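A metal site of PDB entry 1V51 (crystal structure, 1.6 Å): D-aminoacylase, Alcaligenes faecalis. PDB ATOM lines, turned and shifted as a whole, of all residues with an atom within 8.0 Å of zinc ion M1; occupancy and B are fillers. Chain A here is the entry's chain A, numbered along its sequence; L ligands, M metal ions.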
ATOM      1  N   HIS A  80      -4.557 -16.760  34.109  1.00  0.00           N
ATOM      2  CA  HIS A  80      -4.285 -17.816  33.147  1.00  0.00           C
ATOM      3  C   HIS A  80      -2.901 -17.685  32.546  1.00  0.00           C
ATOM      4  O   HIS A  80      -2.688 -16.872  31.639  1.00  0.00           O
ATOM      5  CB  HIS A  80      -5.320 -17.769  32.011  1.00  0.00           C
ATOM      6  CG  HIS A  80      -5.203 -18.919  31.058  1.00  0.00           C
ATOM      7  ND1 HIS A  80      -5.954 -20.068  31.181  1.00  0.00           N
ATOM      8  CD2 HIS A  80      -4.397 -19.109  29.983  1.00  0.00           C
ATOM      9  CE1 HIS A  80      -5.605 -20.921  30.228  1.00  0.00           C
ATOM     10  NE2 HIS A  80      -4.661 -20.367  29.492  1.00  0.00           N
ATOM     11  N   THR A  81      -1.970 -18.473  33.064  1.00  0.00           N
ATOM     12  CA  THR A  81      -0.612 -18.423  32.521  1.00  0.00           C
ATOM     13  C   THR A  81      -0.069 -19.799  32.155  1.00  0.00           C
ATOM     14  O   THR A  81      -0.648 -20.838  32.492  1.00  0.00           O
ATOM     15  CB  THR A  81       0.441 -17.834  33.527  1.00  0.00           C
ATOM     16  OG1 THR A  81       0.866 -18.852  34.457  1.00  0.00           O
ATOM     17  CG2 THR A  81      -0.145 -16.654  34.296  1.00  0.00           C
ATOM     18  N   HIS A  82       1.046 -19.761  31.421  1.00  0.00           N
ATOM     19  CA  HIS A  82       1.795 -20.955  31.083  1.00  0.00           C
ATOM     20  C   HIS A  82       3.232 -20.657  31.521  1.00  0.00           C
ATOM     21  O   HIS A  82       4.201 -20.876  30.779  1.00  0.00           O
ATOM     22  CB  HIS A  82       1.687 -21.263  29.595  1.00  0.00           C
ATOM     23  CG  HIS A  82       0.304 -21.687  29.197  1.00  0.00           C
ATOM     24  ND1 HIS A  82      -0.254 -22.874  29.605  1.00  0.00           N
ATOM     25  CD2 HIS A  82      -0.663 -21.020  28.523  1.00  0.00           C
ATOM     26  CE1 HIS A  82      -1.512 -22.933  29.201  1.00  0.00           C
ATOM     27  NE2 HIS A  82      -1.782 -21.805  28.540  1.00  0.00           N
ATOM     28  N   GLY A 107      -0.086 -24.016  35.198  1.00  0.00           N
ATOM     29  CA  GLY A 107      -0.598 -25.364  34.881  1.00  0.00           C
ATOM     30  C   GLY A 107      -1.997 -25.392  34.293  1.00  0.00           C
ATOM     31  O   GLY A 107      -2.895 -26.127  34.757  1.00  0.00           O
ATOM     32  N   ASN A 108      -2.175 -24.597  33.239  1.00  0.00           N
ATOM     33  CA  ASN A 108      -3.461 -24.449  32.580  1.00  0.00           C
ATOM     34  C   ASN A 108      -3.655 -25.310  31.328  1.00  0.00           C
ATOM     35  O   ASN A 108      -2.696 -25.774  30.718  1.00  0.00           O
ATOM     36  CB  ASN A 108      -3.626 -22.972  32.232  1.00  0.00           C
ATOM     37  CG  ASN A 108      -3.936 -22.146  33.444  1.00  0.00           C
ATOM     38  OD1 ASN A 108      -3.079 -21.417  33.979  1.00  0.00           O
ATOM     39  ND2 ASN A 108      -5.153 -22.271  33.923  1.00  0.00           N
ATOM     40  N   CYS A 109      -4.925 -25.519  30.959  1.00  0.00           N
ATOM     41  CA  CYS A 109      -5.314 -26.261  29.769  1.00  0.00           C
ATOM     42  C   CYS A 109      -4.814 -27.689  29.746  1.00  0.00           C
ATOM     43  O   CYS A 109      -4.580 -28.244  28.659  1.00  0.00           O
ATOM     44  CB  CYS A 109      -4.805 -25.535  28.519  1.00  0.00           C
ATOM     45  SG  CYS A 109      -5.271 -23.776  28.548  1.00  0.00           S
ATOM     46  N   ILE A 111      -2.037 -28.614  30.771  1.00  0.00           N
ATOM     47  CA  ILE A 111      -0.579 -28.541  30.585  1.00  0.00           C
ATOM     48  C   ILE A 111       0.204 -28.078  31.813  1.00  0.00           C
ATOM     49  O   ILE A 111       0.186 -26.891  32.137  1.00  0.00           O
ATOM     50  CB  ILE A 111      -0.213 -27.544  29.457  1.00  0.00           C
ATOM     51  CG1 ILE A 111      -1.005 -27.848  28.175  1.00  0.00           C
ATOM     52  CG2 ILE A 111       1.290 -27.612  29.177  1.00  0.00           C
ATOM     53  CD1 ILE A 111      -0.932 -26.681  27.173  1.00  0.00           C
ATOM     54  N   LEU A 127       5.033 -26.314  24.827  1.00  0.00           N
ATOM     55  CA  LEU A 127       4.948 -24.865  25.023  1.00  0.00           C
ATOM     56  C   LEU A 127       5.684 -24.425  26.292  1.00  0.00           C
ATOM     57  O   LEU A 127       5.971 -23.238  26.465  1.00  0.00           O
ATOM     58  CB  LEU A 127       3.497 -24.412  25.088  1.00  0.00           C
ATOM     59  CG  LEU A 127       2.728 -24.407  23.766  1.00  0.00           C
ATOM     60  CD1 LEU A 127       1.292 -24.010  24.018  1.00  0.00           C
ATOM     61  CD2 LEU A 127       3.394 -23.440  22.776  1.00  0.00           C
ATOM     62  N   TYR A 205      -6.903 -30.600  22.858  1.00  0.00           N
ATOM     63  CA  TYR A 205      -5.578 -31.019  22.363  1.00  0.00           C
ATOM     64  C   TYR A 205      -5.370 -32.526  22.178  1.00  0.00           C
ATOM     65  O   TYR A 205      -5.998 -33.340  22.844  1.00  0.00           O
ATOM     66  CB  TYR A 205      -4.489 -30.448  23.270  1.00  0.00           C
ATOM     67  CG  TYR A 205      -4.413 -28.922  23.189  1.00  0.00           C
ATOM     68  CD1 TYR A 205      -3.955 -28.300  22.040  1.00  0.00           C
ATOM     69  CD2 TYR A 205      -4.832 -28.117  24.260  1.00  0.00           C
ATOM     70  CE1 TYR A 205      -3.906 -26.904  21.935  1.00  0.00           C
ATOM     71  CE2 TYR A 205      -4.797 -26.721  24.164  1.00  0.00           C
ATOM     72  CZ  TYR A 205      -4.325 -26.123  23.004  1.00  0.00           C
ATOM     73  OH  TYR A 205      -4.245 -24.752  22.910  1.00  0.00           O
ATOM     74  N   HIS A 233      -9.753 -25.797  29.358  1.00  0.00           N
ATOM     75  CA  HIS A 233      -9.687 -25.280  28.005  1.00  0.00           C
ATOM     76  C   HIS A 233     -10.764 -26.210  27.441  1.00  0.00           C
ATOM     77  O   HIS A 233     -10.532 -27.409  27.295  1.00  0.00           O
ATOM     78  CB  HIS A 233      -8.334 -25.584  27.357  1.00  0.00           C
ATOM     79  CG  HIS A 233      -8.269 -25.208  25.908  1.00  0.00           C
ATOM     80  ND1 HIS A 233      -7.188 -24.535  25.377  1.00  0.00           N
ATOM     81  CD2 HIS A 233      -9.133 -25.417  24.886  1.00  0.00           C
ATOM     82  CE1 HIS A 233      -7.388 -24.347  24.074  1.00  0.00           C
ATOM     83  NE2 HIS A 233      -8.552 -24.883  23.756  1.00  0.00           N
ATOM     84  N   SER A 262     -11.419 -21.370  30.903  1.00  0.00           N
ATOM     85  CA  SER A 262     -10.260 -20.603  30.427  1.00  0.00           C
ATOM     86  C   SER A 262     -10.459 -19.890  29.104  1.00  0.00           C
ATOM     87  O   SER A 262     -11.123 -20.406  28.206  1.00  0.00           O
ATOM     88  CB  SER A 262      -9.052 -21.526  30.237  1.00  0.00           C
ATOM     89  OG  SER A 262      -8.720 -22.200  31.432  1.00  0.00           O
ATOM     90  N   HIS A 263      -9.797 -18.725  28.995  1.00  0.00           N
ATOM     91  CA  HIS A 263      -9.791 -17.909  27.783  1.00  0.00           C
ATOM     92  C   HIS A 263     -11.070 -18.010  26.972  1.00  0.00           C
ATOM     93  O   HIS A 263     -11.052 -18.479  25.837  1.00  0.00           O
ATOM     94  CB  HIS A 263      -8.541 -18.235  26.902  1.00  0.00           C
ATOM     95  CG  HIS A 263      -8.272 -19.699  26.676  1.00  0.00           C
ATOM     96  ND1 HIS A 263      -9.182 -20.569  26.109  1.00  0.00           N
ATOM     97  CD2 HIS A 263      -7.147 -20.432  26.873  1.00  0.00           C
ATOM     98  CE1 HIS A 263      -8.638 -21.771  25.980  1.00  0.00           C
ATOM     99  NE2 HIS A 263      -7.392 -21.713  26.428  1.00  0.00           N
ATOM    100  N   LYS A 265     -13.996 -17.459  24.545  1.00  0.00           N
ATOM    101  CA  LYS A 265     -14.066 -16.857  23.217  1.00  0.00           C
ATOM    102  C   LYS A 265     -15.016 -17.663  22.342  1.00  0.00           C
ATOM    103  O   LYS A 265     -15.473 -18.750  22.718  1.00  0.00           O
ATOM    104  CB  LYS A 265     -12.688 -16.951  22.555  1.00  0.00           C
ATOM    105  CG  LYS A 265     -12.304 -18.442  22.288  1.00  0.00           C
ATOM    106  CD  LYS A 265     -11.030 -18.604  21.460  1.00  0.00           C
ATOM    107  CE  LYS A 265      -9.801 -18.321  22.249  1.00  0.00           C
ATOM    108  NZ  LYS A 265      -9.555 -19.364  23.325  1.00  0.00           N
ATOM    109  N   ASP A 294     -12.213 -16.612  32.529  1.00  0.00           N
ATOM    110  CA  ASP A 294     -11.264 -15.536  32.303  1.00  0.00           C
ATOM    111  C   ASP A 294     -11.107 -15.357  30.802  1.00  0.00           C
ATOM    112  O   ASP A 294     -11.644 -16.145  29.996  1.00  0.00           O
ATOM    113  CB  ASP A 294      -9.896 -15.748  33.012  1.00  0.00           C
ATOM    114  CG  ASP A 294      -9.151 -16.998  32.578  1.00  0.00           C
ATOM    115  OD1 ASP A 294      -9.027 -17.237  31.354  1.00  0.00           O
ATOM    116  OD2 ASP A 294      -8.645 -17.716  33.478  1.00  0.00           O
ATOM    117  N   TYR A 296      -8.440 -12.998  27.682  1.00  0.00           N
ATOM    118  CA  TYR A 296      -7.354 -12.066  27.400  1.00  0.00           C
ATOM    119  C   TYR A 296      -7.973 -11.041  26.427  1.00  0.00           C
ATOM    120  O   TYR A 296      -8.870 -11.353  25.632  1.00  0.00           O
ATOM    121  CB  TYR A 296      -6.121 -12.787  26.820  1.00  0.00           C
ATOM    122  CG  TYR A 296      -6.397 -13.707  25.669  1.00  0.00           C
ATOM    123  CD1 TYR A 296      -6.540 -13.212  24.370  1.00  0.00           C
ATOM    124  CD2 TYR A 296      -6.519 -15.085  25.881  1.00  0.00           C
ATOM    125  CE1 TYR A 296      -6.794 -14.079  23.293  1.00  0.00           C
ATOM    126  CE2 TYR A 296      -6.774 -15.961  24.821  1.00  0.00           C
ATOM    127  CZ  TYR A 296      -6.909 -15.443  23.535  1.00  0.00           C
ATOM    128  OH  TYR A 296      -7.160 -16.312  22.491  1.00  0.00           O
ATOM    129  N   SER A 302      -3.216 -18.015  20.464  1.00  0.00           N
ATOM    130  CA  SER A 302      -1.875 -18.530  20.212  1.00  0.00           C
ATOM    131  C   SER A 302      -1.688 -19.840  20.965  1.00  0.00           C
ATOM    132  O   SER A 302      -2.110 -19.975  22.110  1.00  0.00           O
ATOM    133  CB  SER A 302      -0.812 -17.511  20.652  1.00  0.00           C
ATOM    134  OG  SER A 302       0.498 -17.951  20.314  1.00  0.00           O
ATOM    135  N   THR A 303      -1.071 -20.826  20.299  1.00  0.00           N
ATOM    136  CA  THR A 303      -0.817 -22.134  20.898  1.00  0.00           C
ATOM    137  C   THR A 303       0.002 -22.937  19.888  1.00  0.00           C
ATOM    138  O   THR A 303       0.609 -22.349  19.013  1.00  0.00           O
ATOM    139  CB  THR A 303      -2.143 -22.877  21.252  1.00  0.00           C
ATOM    140  OG1 THR A 303      -1.810 -24.111  21.895  1.00  0.00           O
ATOM    141  CG2 THR A 303      -2.995 -23.146  20.008  1.00  0.00           C
ATOM    142  N   SER A 378      -3.610 -13.409  30.968  1.00  0.00           N
ATOM    143  CA  SER A 378      -2.807 -13.085  29.787  1.00  0.00           C
ATOM    144  C   SER A 378      -2.635 -14.198  28.744  1.00  0.00           C
ATOM    145  O   SER A 378      -2.547 -13.922  27.527  1.00  0.00           O
ATOM    146  CB  SER A 378      -1.403 -12.618  30.198  1.00  0.00           C
ATOM    147  OG  SER A 378      -0.600 -13.702  30.632  1.00  0.00           O
ATOM    148  N   ASP A 379      -2.570 -15.433  29.223  1.00  0.00           N
ATOM    149  CA  ASP A 379      -2.327 -16.585  28.345  1.00  0.00           C
ATOM    150  C   ASP A 379      -0.975 -16.382  27.633  1.00  0.00           C
ATOM    151  O   ASP A 379      -0.770 -16.848  26.511  1.00  0.00           O
ATOM    152  CB  ASP A 379      -3.446 -16.776  27.317  1.00  0.00           C
ATOM    153  CG  ASP A 379      -3.600 -18.231  26.899  1.00  0.00           C
ATOM    154  OD1 ASP A 379      -2.791 -19.059  27.355  1.00  0.00           O
ATOM    155  OD2 ASP A 379      -4.529 -18.536  26.128  1.00  0.00           O
ATOM    156  N   GLY A 380      -0.057 -15.684  28.280  1.00  0.00           N
ATOM    157  CA  GLY A 380       1.240 -15.494  27.658  1.00  0.00           C
ATOM    158  C   GLY A 380       1.987 -16.821  27.489  1.00  0.00           C
ATOM    159  O   GLY A 380       1.903 -17.705  28.333  1.00  0.00           O
ATOM    160  N   LEU A 381       2.696 -16.971  26.371  1.00  0.00           N
ATOM    161  CA  LEU A 381       3.491 -18.197  26.077  1.00  0.00           C
ATOM    162  C   LEU A 381       4.899 -17.615  26.074  1.00  0.00           C
ATOM    163  O   LEU A 381       5.443 -17.228  25.022  1.00  0.00           O
ATOM    164  CB  LEU A 381       3.082 -18.781  24.719  1.00  0.00           C
ATOM    165  CG  LEU A 381       1.578 -19.096  24.573  1.00  0.00           C
ATOM    166  CD1 LEU A 381       1.292 -19.748  23.245  1.00  0.00           C
ATOM    167  CD2 LEU A 381       1.160 -20.044  25.691  1.00  0.00           C
ATOM    168  N   ARG A 390       0.178 -10.400  24.045  1.00  0.00           N
ATOM    169  CA  ARG A 390      -0.569 -10.516  25.304  1.00  0.00           C
ATOM    170  C   ARG A 390       0.387 -10.850  26.444  1.00  0.00           C
ATOM    171  O   ARG A 390       0.118 -10.563  27.626  1.00  0.00           O
ATOM    172  CB  ARG A 390      -1.664 -11.595  25.181  1.00  0.00           C
ATOM    173  CG  ARG A 390      -1.143 -13.011  24.950  1.00  0.00           C
ATOM    174  CD  ARG A 390      -2.278 -13.909  24.457  1.00  0.00           C
ATOM    175  NE  ARG A 390      -1.898 -15.320  24.434  1.00  0.00           N
ATOM    176  CZ  ARG A 390      -2.655 -16.279  23.899  1.00  0.00           C
ATOM    177  NH1 ARG A 390      -3.810 -15.974  23.330  1.00  0.00           N
ATOM    178  NH2 ARG A 390      -2.272 -17.546  23.997  1.00  0.00           N
HETATM  179  C1  LIG L   1      -3.773 -22.409  25.503  1.00  0.00           C
HETATM  180  O1  LIG L   1      -4.475 -23.340  25.053  1.00  0.00           O
HETATM  181  O2  LIG L   1      -4.219 -21.553  26.282  1.00  0.00           O
HETATM  182  C2  LIG L   1      -2.361 -22.242  24.990  1.00  0.00           C
HETATM  183 ZN    ZN M   1      -3.462 -20.815  27.922  1.00  0.00          ZN
HETATM  184 ZN    ZN M   2      -6.035 -23.248  26.460  1.00  0.00          ZN
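The guanidinium group of Arg 390 is in salt-bridge range of the side-chain carboxylate of Asp 379 (3.3 Å).
N of His 263 lies within hydrogen-bond range of OD1 of Asp 294 (2.9 Å).
The side-chain amino group (NZ) of Lys 265 sits at hydrogen-bond distance from the backbone carbonyl oxygen (O) of His 263 (3.1 Å).
Residues that only touch zinc ion M1: Cys 109 and His 263.
The nearest printed residue that does not touch zinc ion M1 is Asn 108 (4.8 Å).
An oxygen (O2) of the ligand is bound to zinc ion M1.
The side-chain carboxylate (OD1) of Asp 379 is bound to zinc ion M1.
NE2 of His 80 binds zinc ion M1 (2.0 Å).
Zinc ion M1 is bound by NE2 of His 82.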
